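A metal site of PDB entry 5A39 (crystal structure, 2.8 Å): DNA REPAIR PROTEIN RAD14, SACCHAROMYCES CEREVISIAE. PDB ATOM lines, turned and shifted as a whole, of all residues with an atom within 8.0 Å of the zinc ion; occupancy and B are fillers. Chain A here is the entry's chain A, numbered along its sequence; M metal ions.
SG of Cys 26 sits close to ND2 of Asn 10.
O of Asn 10 lies within hydrogen-bond range of N of Cys 4 (2.9 Å).
The backbone NH of Glu 6 sits close to the side-chain sulfur of Cys 4.
The side-chain sulfur of Cys 7 sits close to the backbone NH of Asn 10 (3.4 Å).
SG of Cys 7 sits close to N of Ile 9 (3.6 Å).
Within 4 Å of the zinc ion: Cys 4, Cys 7, Cys 26 and Cys 29.
The nearest printed residue that does not touch the zinc ion is Asn 10 (4.4 Å).
SG of Cys 26 is bound to the zinc ion, at 2.2 Å.
SG of Cys 4 is bound to the zinc ion (2.2 Å).
The side-chain sulfur (SG) of Cys 29 is bound to the zinc ion (2.3 Å).
SG of Cys 7 is bound to the zinc ion (2.3 Å).
The zinc ion has four donor atoms within binding distance.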
ATOM      1  N   LYS A   3      -6.010 -15.373  -5.098  1.00  0.00           N
ATOM      2  CA  LYS A   3      -6.764 -16.293  -4.234  1.00  0.00           C
ATOM      3  C   LYS A   3      -7.575 -17.331  -5.002  1.00  0.00           C
ATOM      4  O   LYS A   3      -8.159 -17.005  -6.006  1.00  0.00           O
ATOM      5  CB  LYS A   3      -7.744 -15.513  -3.372  1.00  0.00           C
ATOM      6  CG  LYS A   3      -7.102 -14.436  -2.501  1.00  0.00           C
ATOM      7  CD  LYS A   3      -6.442 -15.040  -1.290  1.00  0.00           C
ATOM      8  CE  LYS A   3      -5.283 -14.217  -0.764  1.00  0.00           C
ATOM      9  NZ  LYS A   3      -5.764 -12.993  -0.101  1.00  0.00           N
ATOM     10  N   CYS A   4      -7.669 -18.552  -4.497  1.00  0.00           N
ATOM     11  CA  CYS A   4      -8.535 -19.566  -5.082  1.00  0.00           C
ATOM     12  C   CYS A   4      -9.939 -18.997  -5.397  1.00  0.00           C
ATOM     13  O   CYS A   4     -10.551 -18.367  -4.552  1.00  0.00           O
ATOM     14  CB  CYS A   4      -8.573 -20.852  -4.188  1.00  0.00           C
ATOM     15  SG  CYS A   4     -10.045 -21.862  -4.264  1.00  0.00           S
ATOM     16  N   ILE A   5     -10.419 -19.202  -6.616  1.00  0.00           N
ATOM     17  CA  ILE A   5     -11.681 -18.626  -7.040  1.00  0.00           C
ATOM     18  C   ILE A   5     -12.920 -19.185  -6.388  1.00  0.00           C
ATOM     19  O   ILE A   5     -13.948 -18.563  -6.442  1.00  0.00           O
ATOM     20  CB  ILE A   5     -11.890 -18.765  -8.535  1.00  0.00           C
ATOM     21  CG1 ILE A   5     -11.643 -20.218  -8.965  1.00  0.00           C
ATOM     22  CG2 ILE A   5     -10.917 -17.858  -9.241  1.00  0.00           C
ATOM     23  CD1 ILE A   5     -12.532 -20.730 -10.083  1.00  0.00           C
ATOM     24  N   GLU A   6     -12.848 -20.363  -5.796  1.00  0.00           N
ATOM     25  CA  GLU A   6     -13.962 -20.836  -5.011  1.00  0.00           C
ATOM     26  C   GLU A   6     -13.924 -20.227  -3.613  1.00  0.00           C
ATOM     27  O   GLU A   6     -14.863 -19.545  -3.199  1.00  0.00           O
ATOM     28  CB  GLU A   6     -13.956 -22.355  -4.899  1.00  0.00           C
ATOM     29  CG  GLU A   6     -14.299 -23.078  -6.171  1.00  0.00           C
ATOM     30  CD  GLU A   6     -15.786 -23.070  -6.484  1.00  0.00           C
ATOM     31  OE1 GLU A   6     -16.586 -22.706  -5.613  1.00  0.00           O
ATOM     32  OE2 GLU A   6     -16.167 -23.422  -7.624  1.00  0.00           O
ATOM     33  N   CYS A   7     -12.862 -20.485  -2.843  1.00  0.00           N
ATOM     34  CA  CYS A   7     -12.870 -20.098  -1.452  1.00  0.00           C
ATOM     35  C   CYS A   7     -12.463 -18.636  -1.220  1.00  0.00           C
ATOM     36  O   CYS A   7     -12.804 -18.053  -0.193  1.00  0.00           O
ATOM     37  CB  CYS A   7     -12.016 -21.040  -0.615  1.00  0.00           C
ATOM     38  SG  CYS A   7     -10.257 -21.059  -0.866  1.00  0.00           S
ATOM     39  N   HIS A   8     -11.773 -18.044  -2.171  1.00  0.00           N
ATOM     40  CA  HIS A   8     -11.271 -16.682  -2.017  1.00  0.00           C
ATOM     41  C   HIS A   8     -10.309 -16.478  -0.847  1.00  0.00           C
ATOM     42  O   HIS A   8     -10.099 -15.336  -0.414  1.00  0.00           O
ATOM     43  CB  HIS A   8     -12.419 -15.734  -1.852  1.00  0.00           C
ATOM     44  CG  HIS A   8     -13.466 -15.881  -2.898  1.00  0.00           C
ATOM     45  ND1 HIS A   8     -13.210 -15.644  -4.233  1.00  0.00           N
ATOM     46  CD2 HIS A   8     -14.786 -16.167  -2.805  1.00  0.00           C
ATOM     47  CE1 HIS A   8     -14.330 -15.819  -4.927  1.00  0.00           C
ATOM     48  NE2 HIS A   8     -15.302 -16.118  -4.086  1.00  0.00           N
ATOM     49  N   ILE A   9      -9.704 -17.557  -0.338  1.00  0.00           N
ATOM     50  CA  ILE A   9      -8.914 -17.529   0.903  1.00  0.00           C
ATOM     51  C   ILE A   9      -7.529 -18.089   0.682  1.00  0.00           C
ATOM     52  O   ILE A   9      -6.539 -17.467   1.014  1.00  0.00           O
ATOM     53  CB  ILE A   9      -9.615 -18.337   2.020  1.00  0.00           C
ATOM     54  CG1 ILE A   9     -10.853 -17.579   2.517  1.00  0.00           C
ATOM     55  CG2 ILE A   9      -8.679 -18.608   3.182  1.00  0.00           C
ATOM     56  CD1 ILE A   9     -11.900 -18.456   3.176  1.00  0.00           C
ATOM     57  N   ASN A  10      -7.491 -19.294   0.137  1.00  0.00           N
ATOM     58  CA  ASN A  10      -6.244 -19.999  -0.055  1.00  0.00           C
ATOM     59  C   ASN A  10      -5.442 -19.382  -1.156  1.00  0.00           C
ATOM     60  O   ASN A  10      -6.003 -18.851  -2.123  1.00  0.00           O
ATOM     61  CB  ASN A  10      -6.483 -21.498  -0.320  1.00  0.00           C
ATOM     62  CG  ASN A  10      -6.372 -22.327   0.942  1.00  0.00           C
ATOM     63  OD1 ASN A  10      -5.554 -22.052   1.828  1.00  0.00           O
ATOM     64  ND2 ASN A  10      -7.182 -23.388   1.023  1.00  0.00           N
ATOM     65  N   ILE A  11      -4.112 -19.436  -1.012  1.00  0.00           N
ATOM     66  CA  ILE A  11      -3.235 -18.964  -2.069  1.00  0.00           C
ATOM     67  C   ILE A  11      -2.420 -20.068  -2.743  1.00  0.00           C
ATOM     68  O   ILE A  11      -1.961 -19.805  -3.841  1.00  0.00           O
ATOM     69  CB  ILE A  11      -2.329 -17.802  -1.683  1.00  0.00           C
ATOM     70  CG1 ILE A  11      -1.441 -18.216  -0.514  1.00  0.00           C
ATOM     71  CG2 ILE A  11      -3.171 -16.557  -1.411  1.00  0.00           C
ATOM     72  CD1 ILE A  11      -0.087 -17.511  -0.446  1.00  0.00           C
ATOM     73  N   GLU A  12      -2.242 -21.245  -2.109  1.00  0.00           N
ATOM     74  CA  GLU A  12      -1.667 -22.452  -2.760  1.00  0.00           C
ATOM     75  C   GLU A  12      -2.679 -23.187  -3.610  1.00  0.00           C
ATOM     76  O   GLU A  12      -3.598 -23.797  -3.064  1.00  0.00           O
ATOM     77  CB  GLU A  12      -1.224 -23.531  -1.773  1.00  0.00           C
ATOM     78  CG  GLU A  12      -0.252 -23.108  -0.699  1.00  0.00           C
ATOM     79  CD  GLU A  12       1.006 -22.615  -1.286  1.00  0.00           C
ATOM     80  OE1 GLU A  12       1.274 -23.041  -2.425  1.00  0.00           O
ATOM     81  OE2 GLU A  12       1.708 -21.814  -0.612  1.00  0.00           O
ATOM     82  N   MET A  13      -2.479 -23.206  -4.913  1.00  0.00           N
ATOM     83  CA  MET A  13      -3.416 -23.844  -5.782  1.00  0.00           C
ATOM     84  C   MET A  13      -3.082 -25.303  -5.939  1.00  0.00           C
ATOM     85  O   MET A  13      -1.968 -25.726  -5.628  1.00  0.00           O
ATOM     86  CB  MET A  13      -3.405 -23.160  -7.150  1.00  0.00           C
ATOM     87  CG  MET A  13      -3.702 -21.679  -7.109  1.00  0.00           C
ATOM     88  SD  MET A  13      -5.196 -21.321  -6.174  1.00  0.00           S
ATOM     89  CE  MET A  13      -5.041 -19.562  -5.954  1.00  0.00           C
ATOM     90  N   GLN A  24      -7.341 -21.522 -11.269  1.00  0.00           N
ATOM     91  CA  GLN A  24      -6.858 -21.045  -9.974  1.00  0.00           C
ATOM     92  C   GLN A  24      -7.745 -21.587  -8.881  1.00  0.00           C
ATOM     93  O   GLN A  24      -8.694 -20.918  -8.473  1.00  0.00           O
ATOM     94  CB  GLN A  24      -6.893 -19.549  -9.931  1.00  0.00           C
ATOM     95  CG  GLN A  24      -5.985 -18.967 -10.996  1.00  0.00           C
ATOM     96  CD  GLN A  24      -4.745 -18.338 -10.408  1.00  0.00           C
ATOM     97  OE1 GLN A  24      -4.791 -17.765  -9.292  1.00  0.00           O
ATOM     98  NE2 GLN A  24      -3.612 -18.395 -11.171  1.00  0.00           N
ATOM     99  N   VAL A  25      -7.452 -22.818  -8.448  1.00  0.00           N
ATOM    100  CA  VAL A  25      -8.290 -23.554  -7.489  1.00  0.00           C
ATOM    101  C   VAL A  25      -7.502 -24.429  -6.550  1.00  0.00           C
ATOM    102  O   VAL A  25      -6.595 -25.164  -6.980  1.00  0.00           O
ATOM    103  CB  VAL A  25      -9.308 -24.478  -8.192  1.00  0.00           C
ATOM    104  CG1 VAL A  25     -10.259 -25.105  -7.178  1.00  0.00           C
ATOM    105  CG2 VAL A  25     -10.109 -23.680  -9.211  1.00  0.00           C
ATOM    106  N   CYS A  26      -7.865 -24.367  -5.272  1.00  0.00           N
ATOM    107  CA  CYS A  26      -7.100 -25.096  -4.260  1.00  0.00           C
ATOM    108  C   CYS A  26      -7.539 -26.519  -4.152  1.00  0.00           C
ATOM    109  O   CYS A  26      -8.598 -26.898  -4.588  1.00  0.00           O
ATOM    110  CB  CYS A  26      -7.087 -24.370  -2.909  1.00  0.00           C
ATOM    111  SG  CYS A  26      -8.592 -24.338  -1.946  1.00  0.00           S
ATOM    112  N   LYS A  27      -6.680 -27.325  -3.606  1.00  0.00           N
ATOM    113  CA  LYS A  27      -6.933 -28.752  -3.515  1.00  0.00           C
ATOM    114  C   LYS A  27      -8.227 -28.973  -2.730  1.00  0.00           C
ATOM    115  O   LYS A  27      -9.057 -29.760  -3.139  1.00  0.00           O
ATOM    116  CB  LYS A  27      -5.728 -29.452  -2.846  1.00  0.00           C
ATOM    117  CG  LYS A  27      -5.973 -30.882  -2.374  1.00  0.00           C
ATOM    118  CD  LYS A  27      -5.574 -31.887  -3.433  1.00  0.00           C
ATOM    119  CE  LYS A  27      -4.064 -32.117  -3.411  1.00  0.00           C
ATOM    120  NZ  LYS A  27      -3.673 -33.456  -3.986  1.00  0.00           N
ATOM    121  N   GLN A  28      -8.411 -28.289  -1.612  1.00  0.00           N
ATOM    122  CA  GLN A  28      -9.542 -28.552  -0.767  1.00  0.00           C
ATOM    123  C   GLN A  28     -10.846 -28.189  -1.460  1.00  0.00           C
ATOM    124  O   GLN A  28     -11.791 -28.938  -1.380  1.00  0.00           O
ATOM    125  CB  GLN A  28      -9.386 -27.747   0.485  1.00  0.00           C
ATOM    126  CG  GLN A  28     -10.502 -27.824   1.493  1.00  0.00           C
ATOM    127  CD  GLN A  28     -10.217 -26.979   2.728  1.00  0.00           C
ATOM    128  OE1 GLN A  28      -9.084 -26.499   2.960  1.00  0.00           O
ATOM    129  NE2 GLN A  28     -11.221 -26.789   3.508  1.00  0.00           N
ATOM    130  N   CYS A  29     -10.862 -27.034  -2.115  1.00  0.00           N
ATOM    131  CA  CYS A  29     -12.040 -26.531  -2.803  1.00  0.00           C
ATOM    132  C   CYS A  29     -12.330 -27.438  -3.956  1.00  0.00           C
ATOM    133  O   CYS A  29     -13.485 -27.660  -4.302  1.00  0.00           O
ATOM    134  CB  CYS A  29     -11.825 -25.155  -3.344  1.00  0.00           C
ATOM    135  SG  CYS A  29     -12.288 -23.848  -2.233  1.00  0.00           S
ATOM    136  N   SER A  30     -11.313 -28.011  -4.562  1.00  0.00           N
ATOM    137  CA  SER A  30     -11.575 -29.006  -5.598  1.00  0.00           C
ATOM    138  C   SER A  30     -12.266 -30.283  -5.085  1.00  0.00           C
ATOM    139  O   SER A  30     -13.129 -30.784  -5.759  1.00  0.00           O
ATOM    140  CB  SER A  30     -10.307 -29.374  -6.378  1.00  0.00           C
ATOM    141  OG  SER A  30      -9.713 -30.537  -5.886  1.00  0.00           O
ATOM    142  N   GLU A  32     -14.174 -30.392  -2.431  1.00  0.00           N
ATOM    143  CA  GLU A  32     -15.508 -29.921  -2.005  1.00  0.00           C
ATOM    144  C   GLU A  32     -16.446 -29.572  -3.185  1.00  0.00           C
ATOM    145  O   GLU A  32     -17.569 -29.111  -2.965  1.00  0.00           O
ATOM    146  CB  GLU A  32     -15.359 -28.705  -1.049  1.00  0.00           C
ATOM    147  CG  GLU A  32     -14.613 -28.998   0.267  1.00  0.00           C
ATOM    148  CD  GLU A  32     -14.301 -27.735   1.126  1.00  0.00           C
ATOM    149  OE1 GLU A  32     -13.910 -26.676   0.545  1.00  0.00           O
ATOM    150  OE2 GLU A  32     -14.421 -27.799   2.391  1.00  0.00           O
ATOM    151  N   HIS A  33     -16.002 -29.772  -4.425  1.00  0.00           N
ATOM    152  CA  HIS A  33     -16.835 -29.437  -5.598  1.00  0.00           C
ATOM    153  C   HIS A  33     -16.576 -30.361  -6.811  1.00  0.00           C
ATOM    154  O   HIS A  33     -16.138 -29.916  -7.883  1.00  0.00           O
ATOM    155  CB  HIS A  33     -16.603 -27.976  -5.997  1.00  0.00           C
ATOM    156  CG  HIS A  33     -16.989 -26.966  -4.955  1.00  0.00           C
ATOM    157  ND1 HIS A  33     -18.295 -26.580  -4.735  1.00  0.00           N
ATOM    158  CD2 HIS A  33     -16.238 -26.211  -4.118  1.00  0.00           C
ATOM    159  CE1 HIS A  33     -18.332 -25.640  -3.810  1.00  0.00           C
ATOM    160  NE2 HIS A  33     -17.104 -25.392  -3.423  1.00  0.00           N
HETATM  161 ZN    ZN M   1     -10.204 -22.893  -2.272  1.00  0.00          ZN
